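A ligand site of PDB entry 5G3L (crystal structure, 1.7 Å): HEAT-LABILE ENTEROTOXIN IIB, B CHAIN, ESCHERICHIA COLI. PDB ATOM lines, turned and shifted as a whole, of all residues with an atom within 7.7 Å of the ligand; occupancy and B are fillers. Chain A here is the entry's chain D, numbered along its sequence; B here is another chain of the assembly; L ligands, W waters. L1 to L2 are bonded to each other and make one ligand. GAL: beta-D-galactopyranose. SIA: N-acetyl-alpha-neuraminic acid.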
ATOM      1  N   ASP A  29      -7.784   9.371 -16.067  1.00  0.00           N
ATOM      2  CA  ASP A  29      -6.876   9.676 -14.943  1.00  0.00           C
ATOM      3  C   ASP A  29      -6.469  11.137 -14.970  1.00  0.00           C
ATOM      4  O   ASP A  29      -6.025  11.648 -15.999  1.00  0.00           O
ATOM      5  CB  ASP A  29      -5.687   8.720 -15.072  1.00  0.00           C
ATOM      6  CG  ASP A  29      -4.678   8.802 -13.939  1.00  0.00           C
ATOM      7  OD1 ASP A  29      -4.499   9.861 -13.316  1.00  0.00           O
ATOM      8  OD2 ASP A  29      -4.011   7.751 -13.666  1.00  0.00           O
ATOM      9  N   ILE A  30      -6.652  11.840 -13.822  1.00  0.00           N
ATOM     10  CA  ILE A  30      -6.189  13.235 -13.726  1.00  0.00           C
ATOM     11  C   ILE A  30      -5.031  13.438 -12.729  1.00  0.00           C
ATOM     12  O   ILE A  30      -4.668  14.569 -12.423  1.00  0.00           O
ATOM     13  CB  ILE A  30      -7.274  14.255 -13.430  1.00  0.00           C
ATOM     14  CG1 ILE A  30      -7.993  13.944 -12.095  1.00  0.00           C
ATOM     15  CG2 ILE A  30      -8.256  14.296 -14.591  1.00  0.00           C
ATOM     16  CD1 ILE A  30      -8.774  15.189 -11.632  1.00  0.00           C
ATOM     17  N   ASN A  31      -4.445  12.360 -12.280  1.00  0.00           N
ATOM     18  CA  ASN A  31      -3.362  12.438 -11.275  1.00  0.00           C
ATOM     19  C   ASN A  31      -2.107  12.999 -11.923  1.00  0.00           C
ATOM     20  O   ASN A  31      -1.887  12.829 -13.121  1.00  0.00           O
ATOM     21  CB  ASN A  31      -3.116  11.034 -10.652  1.00  0.00           C
ATOM     22  CG  ASN A  31      -4.095  10.742  -9.510  1.00  0.00           C
ATOM     23  OD1 ASN A  31      -4.370  11.602  -8.690  1.00  0.00           O
ATOM     24  ND2 ASN A  31      -4.530   9.539  -9.439  1.00  0.00           N
ATOM     25  N   ASN A  32      -1.264  13.653 -11.123  1.00  0.00           N
ATOM     26  CA  ASN A  32      -0.006  14.191 -11.670  1.00  0.00           C
ATOM     27  C   ASN A  32       0.813  13.103 -12.339  1.00  0.00           C
ATOM     28  O   ASN A  32       0.943  12.016 -11.813  1.00  0.00           O
ATOM     29  CB  ASN A  32       0.939  14.750 -10.577  1.00  0.00           C
ATOM     30  CG  ASN A  32       0.349  15.835  -9.730  1.00  0.00           C
ATOM     31  OD1 ASN A  32       0.836  16.117  -8.576  1.00  0.00           O
ATOM     32  ND2 ASN A  32      -0.668  16.478 -10.220  1.00  0.00           N
ATOM     33  N   ASN A  33       1.368  13.390 -13.506  1.00  0.00           N
ATOM     34  CA  ASN A  33       2.283  12.432 -14.209  1.00  0.00           C
ATOM     35  C   ASN A  33       1.657  11.214 -14.834  1.00  0.00           C
ATOM     36  O   ASN A  33       2.264  10.654 -15.732  1.00  0.00           O
ATOM     37  CB  ASN A  33       3.398  11.937 -13.282  1.00  0.00           C
ATOM     38  CG  ASN A  33       4.245  13.067 -12.729  1.00  0.00           C
ATOM     39  OD1 ASN A  33       4.611  13.031 -11.557  1.00  0.00           O
ATOM     40  ND2 ASN A  33       4.535  14.082 -13.530  1.00  0.00           N
ATOM     41  N   THR A  34       0.471  10.780 -14.368  1.00  0.00           N
ATOM     42  CA  THR A  34      -0.201   9.685 -15.012  1.00  0.00           C
ATOM     43  C   THR A  34      -1.464  10.114 -15.762  1.00  0.00           C
ATOM     44  O   THR A  34      -2.196   9.286 -16.294  1.00  0.00           O
ATOM     45  CB  THR A  34      -0.559   8.563 -14.051  1.00  0.00           C
ATOM     46  OG1 THR A  34      -1.414   9.055 -13.021  1.00  0.00           O
ATOM     47  CG2 THR A  34       0.703   7.980 -13.446  1.00  0.00           C
ATOM     48  N   ASP A  35      -1.693  11.407 -15.795  1.00  0.00           N
ATOM     49  CA  ASP A  35      -2.905  11.961 -16.386  1.00  0.00           C
ATOM     50  C   ASP A  35      -3.045  11.515 -17.864  1.00  0.00           C
ATOM     51  O   ASP A  35      -2.076  11.559 -18.637  1.00  0.00           O
ATOM     52  CB  ASP A  35      -2.921  13.462 -16.246  1.00  0.00           C
ATOM     53  CG  ASP A  35      -1.894  14.166 -17.081  1.00  0.00           C
ATOM     54  OD1 ASP A  35      -0.722  14.053 -16.784  1.00  0.00           O
ATOM     55  OD2 ASP A  35      -2.325  14.926 -17.998  1.00  0.00           O
ATOM     56  N   ASN B   9      -0.553   3.121 -10.795  1.00  0.00           N
ATOM     57  CA  ASN B   9      -0.756   4.551 -10.865  1.00  0.00           C
ATOM     58  C   ASN B   9      -1.418   5.126  -9.556  1.00  0.00           C
ATOM     59  O   ASN B   9      -0.972   6.124  -9.032  1.00  0.00           O
ATOM     60  CB  ASN B   9      -1.584   4.948 -12.083  1.00  0.00           C
ATOM     61  CG  ASN B   9      -0.882   4.628 -13.390  1.00  0.00           C
ATOM     62  OD1 ASN B   9       0.336   4.486 -13.441  1.00  0.00           O
ATOM     63  ND2 ASN B   9      -1.664   4.571 -14.459  1.00  0.00           N
ATOM     64  N   CYS B  10      -2.412   4.424  -9.011  1.00  0.00           N
ATOM     65  CA  CYS B  10      -3.075   4.860  -7.763  1.00  0.00           C
ATOM     66  C   CYS B  10      -2.102   4.758  -6.568  1.00  0.00           C
ATOM     67  O   CYS B  10      -2.083   5.630  -5.667  1.00  0.00           O
ATOM     68  CB  CYS B  10      -4.343   4.050  -7.485  1.00  0.00           C
ATOM     69  SG  CYS B  10      -5.376   4.906  -6.215  1.00  0.00           S
ATOM     70  N   ASN B  11      -1.268   3.724  -6.630  1.00  0.00           N
ATOM     71  CA  ASN B  11      -0.270   3.456  -5.549  1.00  0.00           C
ATOM     72  C   ASN B  11       0.774   4.566  -5.389  1.00  0.00           C
ATOM     73  O   ASN B  11       1.367   4.696  -4.326  1.00  0.00           O
ATOM     74  CB  ASN B  11       0.403   2.084  -5.713  1.00  0.00           C
ATOM     75  CG  ASN B  11      -0.514   0.890  -5.359  1.00  0.00           C
ATOM     76  OD1 ASN B  11      -1.604   1.047  -4.844  1.00  0.00           O
ATOM     77  ND2 ASN B  11      -0.073  -0.305  -5.680  1.00  0.00           N
ATOM     78  N   ARG B  12       0.950   5.389  -6.423  1.00  0.00           N
ATOM     79  CA  ARG B  12       1.837   6.539  -6.363  1.00  0.00           C
ATOM     80  C   ARG B  12       1.255   7.687  -5.525  1.00  0.00           C
ATOM     81  O   ARG B  12       1.968   8.636  -5.227  1.00  0.00           O
ATOM     82  CB  ARG B  12       2.108   7.156  -7.734  1.00  0.00           C
ATOM     83  CG  ARG B  12       2.810   6.281  -8.757  1.00  0.00           C
ATOM     84  CD  ARG B  12       3.365   7.229  -9.832  1.00  0.00           C
ATOM     85  NE  ARG B  12       3.405   6.652 -11.150  1.00  0.00           N
ATOM     86  CZ  ARG B  12       3.803   7.321 -12.229  1.00  0.00           C
ATOM     87  NH1 ARG B  12       4.234   8.584 -12.149  1.00  0.00           N
ATOM     88  NH2 ARG B  12       3.793   6.712 -13.414  1.00  0.00           N
ATOM     89  N   THR B  13      -0.030   7.614  -5.197  1.00  0.00           N
ATOM     90  CA  THR B  13      -0.732   8.762  -4.627  1.00  0.00           C
ATOM     91  C   THR B  13      -1.246   8.477  -3.192  1.00  0.00           C
ATOM     92  O   THR B  13      -1.192   7.365  -2.716  1.00  0.00           O
ATOM     93  CB  THR B  13      -1.976   9.169  -5.485  1.00  0.00           C
ATOM     94  OG1 THR B  13      -3.011   8.214  -5.271  1.00  0.00           O
ATOM     95  CG2 THR B  13      -1.627   9.218  -6.962  1.00  0.00           C
ATOM     96  N   THR B  14      -1.788   9.540  -2.611  1.00  0.00           N
ATOM     97  CA  THR B  14      -2.454   9.524  -1.278  1.00  0.00           C
ATOM     98  C   THR B  14      -3.873   9.012  -1.348  1.00  0.00           C
ATOM     99  O   THR B  14      -4.527   8.812  -0.313  1.00  0.00           O
ATOM    100  CB  THR B  14      -2.513  10.916  -0.653  1.00  0.00           C
ATOM    101  OG1 THR B  14      -3.210  11.831  -1.509  1.00  0.00           O
ATOM    102  CG2 THR B  14      -1.121  11.458  -0.411  1.00  0.00           C
ATOM    103  N   ALA B  15      -4.360   8.799  -2.567  1.00  0.00           N
ATOM    104  CA  ALA B  15      -5.698   8.244  -2.772  1.00  0.00           C
ATOM    105  C   ALA B  15      -5.810   6.770  -2.527  1.00  0.00           C
ATOM    106  O   ALA B  15      -4.809   6.060  -2.446  1.00  0.00           O
ATOM    107  CB  ALA B  15      -6.233   8.656  -4.144  1.00  0.00           C
ATOM    108  N   SER B  50     -14.559  14.574 -10.228  1.00  0.00           N
ATOM    109  CA  SER B  50     -13.735  15.783 -10.477  1.00  0.00           C
ATOM    110  C   SER B  50     -14.276  16.623 -11.648  1.00  0.00           C
ATOM    111  O   SER B  50     -14.899  16.129 -12.553  1.00  0.00           O
ATOM    112  CB  SER B  50     -12.256  15.406 -10.782  1.00  0.00           C
ATOM    113  OG  SER B  50     -11.562  14.852  -9.628  1.00  0.00           O
ATOM    114  N   ASP B  57      -7.594  18.792 -18.610  1.00  0.00           N
ATOM    115  CA  ASP B  57      -8.378  18.072 -17.607  1.00  0.00           C
ATOM    116  C   ASP B  57      -9.861  18.106 -17.946  1.00  0.00           C
ATOM    117  O   ASP B  57     -10.638  17.276 -17.429  1.00  0.00           O
ATOM    118  CB  ASP B  57      -8.123  18.531 -16.164  1.00  0.00           C
ATOM    119  CG  ASP B  57      -6.784  18.046 -15.618  1.00  0.00           C
ATOM    120  OD1 ASP B  57      -6.153  17.191 -16.232  1.00  0.00           O
ATOM    121  OD2 ASP B  57      -6.364  18.563 -14.564  1.00  0.00           O
ATOM    122  N   MET B  64     -14.838  10.893 -17.267  1.00  0.00           N
ATOM    123  CA  MET B  64     -15.313  10.339 -15.988  1.00  0.00           C
ATOM    124  C   MET B  64     -16.870  10.329 -15.899  1.00  0.00           C
ATOM    125  O   MET B  64     -17.435   9.359 -15.384  1.00  0.00           O
ATOM    126  CB  MET B  64     -14.747  11.135 -14.782  1.00  0.00           C
ATOM    127  CG  MET B  64     -13.246  10.988 -14.653  1.00  0.00           C
ATOM    128  SD  MET B  64     -12.729  11.893 -13.136  1.00  0.00           S
ATOM    129  CE  MET B  64     -10.962  11.401 -13.040  1.00  0.00           C
ATOM    130  N   SER B  83      -9.577  10.179  -3.419  1.00  0.00           N
ATOM    131  CA  SER B  83      -8.917  10.830  -2.273  1.00  0.00           C
ATOM    132  C   SER B  83      -9.841  10.805  -1.019  1.00  0.00           C
ATOM    133  O   SER B  83     -10.954  11.305  -1.089  1.00  0.00           O
ATOM    134  CB  SER B  83      -8.597  12.231  -2.618  1.00  0.00           C
ATOM    135  OG  SER B  83      -8.144  12.939  -1.457  1.00  0.00           O
ATOM    136  N   ALA B  85      -9.412  12.748   1.482  1.00  0.00           N
ATOM    137  CA  ALA B  85      -9.209  14.047   2.127  1.00  0.00           C
ATOM    138  C   ALA B  85     -10.479  14.845   2.289  1.00  0.00           C
ATOM    139  O   ALA B  85     -10.573  15.733   3.143  1.00  0.00           O
ATOM    140  CB  ALA B  85      -8.198  14.882   1.385  1.00  0.00           C
ATOM    141  N   VAL B  90     -13.265  12.341  -3.489  1.00  0.00           N
ATOM    142  CA  VAL B  90     -13.129  12.825  -4.897  1.00  0.00           C
ATOM    143  C   VAL B  90     -12.362  11.816  -5.786  1.00  0.00           C
ATOM    144  O   VAL B  90     -11.351  11.257  -5.378  1.00  0.00           O
ATOM    145  CB  VAL B  90     -12.429  14.184  -4.972  1.00  0.00           C
ATOM    146  CG1 VAL B  90     -12.323  14.684  -6.396  1.00  0.00           C
ATOM    147  CG2 VAL B  90     -13.220  15.182  -4.141  1.00  0.00           C
ATOM    148  N   ILE B  91     -12.969  11.542  -6.937  1.00  0.00           N
ATOM    149  CA  ILE B  91     -12.396  10.593  -7.901  1.00  0.00           C
ATOM    150  C   ILE B  91     -11.294  11.233  -8.694  1.00  0.00           C
ATOM    151  O   ILE B  91     -11.534  12.210  -9.423  1.00  0.00           O
ATOM    152  CB  ILE B  91     -13.473  10.029  -8.843  1.00  0.00           C
ATOM    153  CG1 ILE B  91     -14.492   9.233  -8.093  1.00  0.00           C
ATOM    154  CG2 ILE B  91     -12.858   9.119  -9.899  1.00  0.00           C
ATOM    155  CD1 ILE B  91     -15.815   9.021  -8.836  1.00  0.00           C
ATOM    156  N   TRP B  92     -10.113  10.674  -8.542  1.00  0.00           N
ATOM    157  CA  TRP B  92      -8.893  11.119  -9.287  1.00  0.00           C
ATOM    158  C   TRP B  92      -8.559  10.258 -10.520  1.00  0.00           C
ATOM    159  O   TRP B  92      -7.929  10.765 -11.451  1.00  0.00           O
ATOM    160  CB  TRP B  92      -7.688  11.241  -8.363  1.00  0.00           C
ATOM    161  CG  TRP B  92      -7.747  12.352  -7.390  1.00  0.00           C
ATOM    162  CD1 TRP B  92      -8.577  13.423  -7.397  1.00  0.00           C
ATOM    163  CD2 TRP B  92      -6.808  12.570  -6.305  1.00  0.00           C
ATOM    164  NE1 TRP B  92      -8.281  14.267  -6.350  1.00  0.00           N
ATOM    165  CE2 TRP B  92      -7.205  13.749  -5.660  1.00  0.00           C
ATOM    166  CE3 TRP B  92      -5.729  11.857  -5.802  1.00  0.00           C
ATOM    167  CZ2 TRP B  92      -6.500  14.280  -4.542  1.00  0.00           C
ATOM    168  CZ3 TRP B  92      -5.050  12.366  -4.682  1.00  0.00           C
ATOM    169  CH2 TRP B  92      -5.432  13.581  -4.090  1.00  0.00           C
ATOM    170  N   ALA B  93      -9.031   9.038 -10.511  1.00  0.00           N
ATOM    171  CA  ALA B  93      -8.977   8.143 -11.682  1.00  0.00           C
ATOM    172  C   ALA B  93     -10.073   7.126 -11.553  1.00  0.00           C
ATOM    173  O   ALA B  93     -10.473   6.719 -10.446  1.00  0.00           O
ATOM    174  CB  ALA B  93      -7.613   7.454 -11.785  1.00  0.00           C
HETATM  175  C1  GAL L   1       2.268  16.996  -2.281  1.00  0.00           C
HETATM  176  C2  GAL L   1       1.969  16.219  -3.519  1.00  0.00           C
HETATM  177  C3  GAL L   1       0.840  15.257  -3.295  1.00  0.00           C
HETATM  178  C4  GAL L   1       1.289  14.405  -2.163  1.00  0.00           C
HETATM  179  C5  GAL L   1       1.555  15.229  -0.935  1.00  0.00           C
HETATM  180  C6  GAL L   1       1.877  14.274   0.181  1.00  0.00           C
HETATM  181  O1  GAL L   1       3.351  17.856  -2.653  1.00  0.00           O
HETATM  182  O2  GAL L   1       1.747  17.175  -4.520  1.00  0.00           O
HETATM  183  O3  GAL L   1       0.805  14.388  -4.386  1.00  0.00           O
HETATM  184  O4  GAL L   1       2.492  13.864  -2.681  1.00  0.00           O
HETATM  185  O5  GAL L   1       2.638  16.101  -1.247  1.00  0.00           O
HETATM  186  O6  GAL L   1       1.205  14.626   1.367  1.00  0.00           O
HETATM  187  C1  SIA L   2      -1.173  13.188  -3.927  1.00  0.00           C
HETATM  188  C2  SIA L   2      -0.525  14.110  -4.885  1.00  0.00           C
HETATM  189  C3  SIA L   2      -0.394  13.476  -6.287  1.00  0.00           C
HETATM  190  C4  SIA L   2      -1.761  13.379  -6.958  1.00  0.00           C
HETATM  191  C5  SIA L   2      -2.470  14.710  -6.977  1.00  0.00           C
HETATM  192  C6  SIA L   2      -2.594  15.221  -5.509  1.00  0.00           C
HETATM  193  C7  SIA L   2      -3.311  16.536  -5.301  1.00  0.00           C
HETATM  194  C8  SIA L   2      -3.055  17.089  -3.895  1.00  0.00           C
HETATM  195  C9  SIA L   2      -3.806  18.354  -3.519  1.00  0.00           C
HETATM  196  C10 SIA L   2      -4.347  15.475  -8.364  1.00  0.00           C
HETATM  197  C11 SIA L   2      -5.672  15.053  -8.964  1.00  0.00           C
HETATM  198  N5  SIA L   2      -3.774  14.546  -7.609  1.00  0.00           N
HETATM  199  O1A SIA L   2      -0.940  11.959  -4.007  1.00  0.00           O
HETATM  200  O1B SIA L   2      -1.838  13.724  -2.996  1.00  0.00           O
HETATM  201  O4  SIA L   2      -1.527  12.906  -8.278  1.00  0.00           O
HETATM  202  O6  SIA L   2      -1.244  15.323  -5.004  1.00  0.00           O
HETATM  203  O7  SIA L   2      -2.790  17.438  -6.254  1.00  0.00           O
HETATM  204  O8  SIA L   2      -3.307  16.049  -2.979  1.00  0.00           O
HETATM  205  O9  SIA L   2      -5.224  18.147  -3.676  1.00  0.00           O
HETATM  206  O10 SIA L   2      -3.916  16.593  -8.582  1.00  0.00           O
HETATM  207  O   HOH W   1      -7.130  16.827  -1.827  1.00  0.00           O
HETATM  208  O   HOH W   2       0.023  18.064  -6.692  1.00  0.00           O
HETATM  209  O   HOH W   3       1.988  11.654  -4.317  1.00  0.00           O
HETATM  210  O   HOH W   4      -2.983  16.412 -11.273  1.00  0.00           O
HETATM  211  O   HOH W   5       0.518  10.900  -9.366  1.00  0.00           O
HETATM  212  O   HOH W   6      -6.908  17.614  -5.573  1.00  0.00           O
HETATM  213  O   HOH W   7       3.029  13.645  -5.593  1.00  0.00           O
HETATM  214  O   HOH W   8      -3.754  20.738  -6.737  1.00  0.00           O
HETATM  215  O   HOH W   9       1.950  14.065   3.665  1.00  0.00           O
HETATM  216  O   HOH W  10      -5.120  15.574  -0.806  1.00  0.00           O
HETATM  217  O   HOH W  11      -7.271  20.207  -3.192  1.00  0.00           O
HETATM  218  O   HOH W  12      -4.219  18.494 -10.294  1.00  0.00           O
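The backbone NH of Thr 14 of chain B lies within hydrogen-bond range of an oxygen (O1A) of SIA L2.
O1B of SIA L2 lies within hydrogen-bond range of OG1 of Thr 14 of chain B, 2.8 Å away.
An oxygen (O4) of SIA L2 lies within hydrogen-bond range of the backbone NH (N) of Asn 32 (3.0 Å).
The side-chain amide oxygen of Asn 31 is in hydrogen-bond range of an oxygen (O4) of SIA L2 (3.2 Å).
The backbone NH of Asn 31 sits at hydrogen-bond distance from the side-chain carboxylate of Asp 29.
The backbone NH of Ala 15 of chain B is in hydrogen-bond range of the side-chain hydroxyl of Thr 13 of chain B, 3.1 Å away.
The backbone carbonyl oxygen (O) of Cys 10 of chain B lies within hydrogen-bond range of the side-chain hydroxyl (OG1) of Thr 13 of chain B (2.8 Å).
O of Trp 92 of chain B is in hydrogen-bond range of N of Ile 30 (2.9 Å).
Residues that only touch the ligand: Thr 13 of chain B (3.3 Å), Trp 92 of chain B (3.4 Å) and Ile 30 (3.6 Å).
Hydrophobic or aromatic side chains within 4 Å of the ligand: Trp 92 of chain B.
The nearest printed residue that does not touch the ligand is Arg 12 of chain B (4.6 Å).
Water W3 lies within hydrogen-bond range of O4 of GAL L1 (2.8 Å) and O of Arg 12 of chain B (3.2 Å).
Water W4 lies within hydrogen-bond range of ND2 of Asn 32 (2.5 Å), O of Ile 30 (2.7 Å) and O10 of SIA L2 (2.9 Å).
Water W2 bridges the side-chain amide oxygen (OD1) of Asn 32 and an oxygen (O2) of GAL L1.
Water W5 lies within hydrogen-bond range of O of Asn 32 and O4 of SIA L2.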
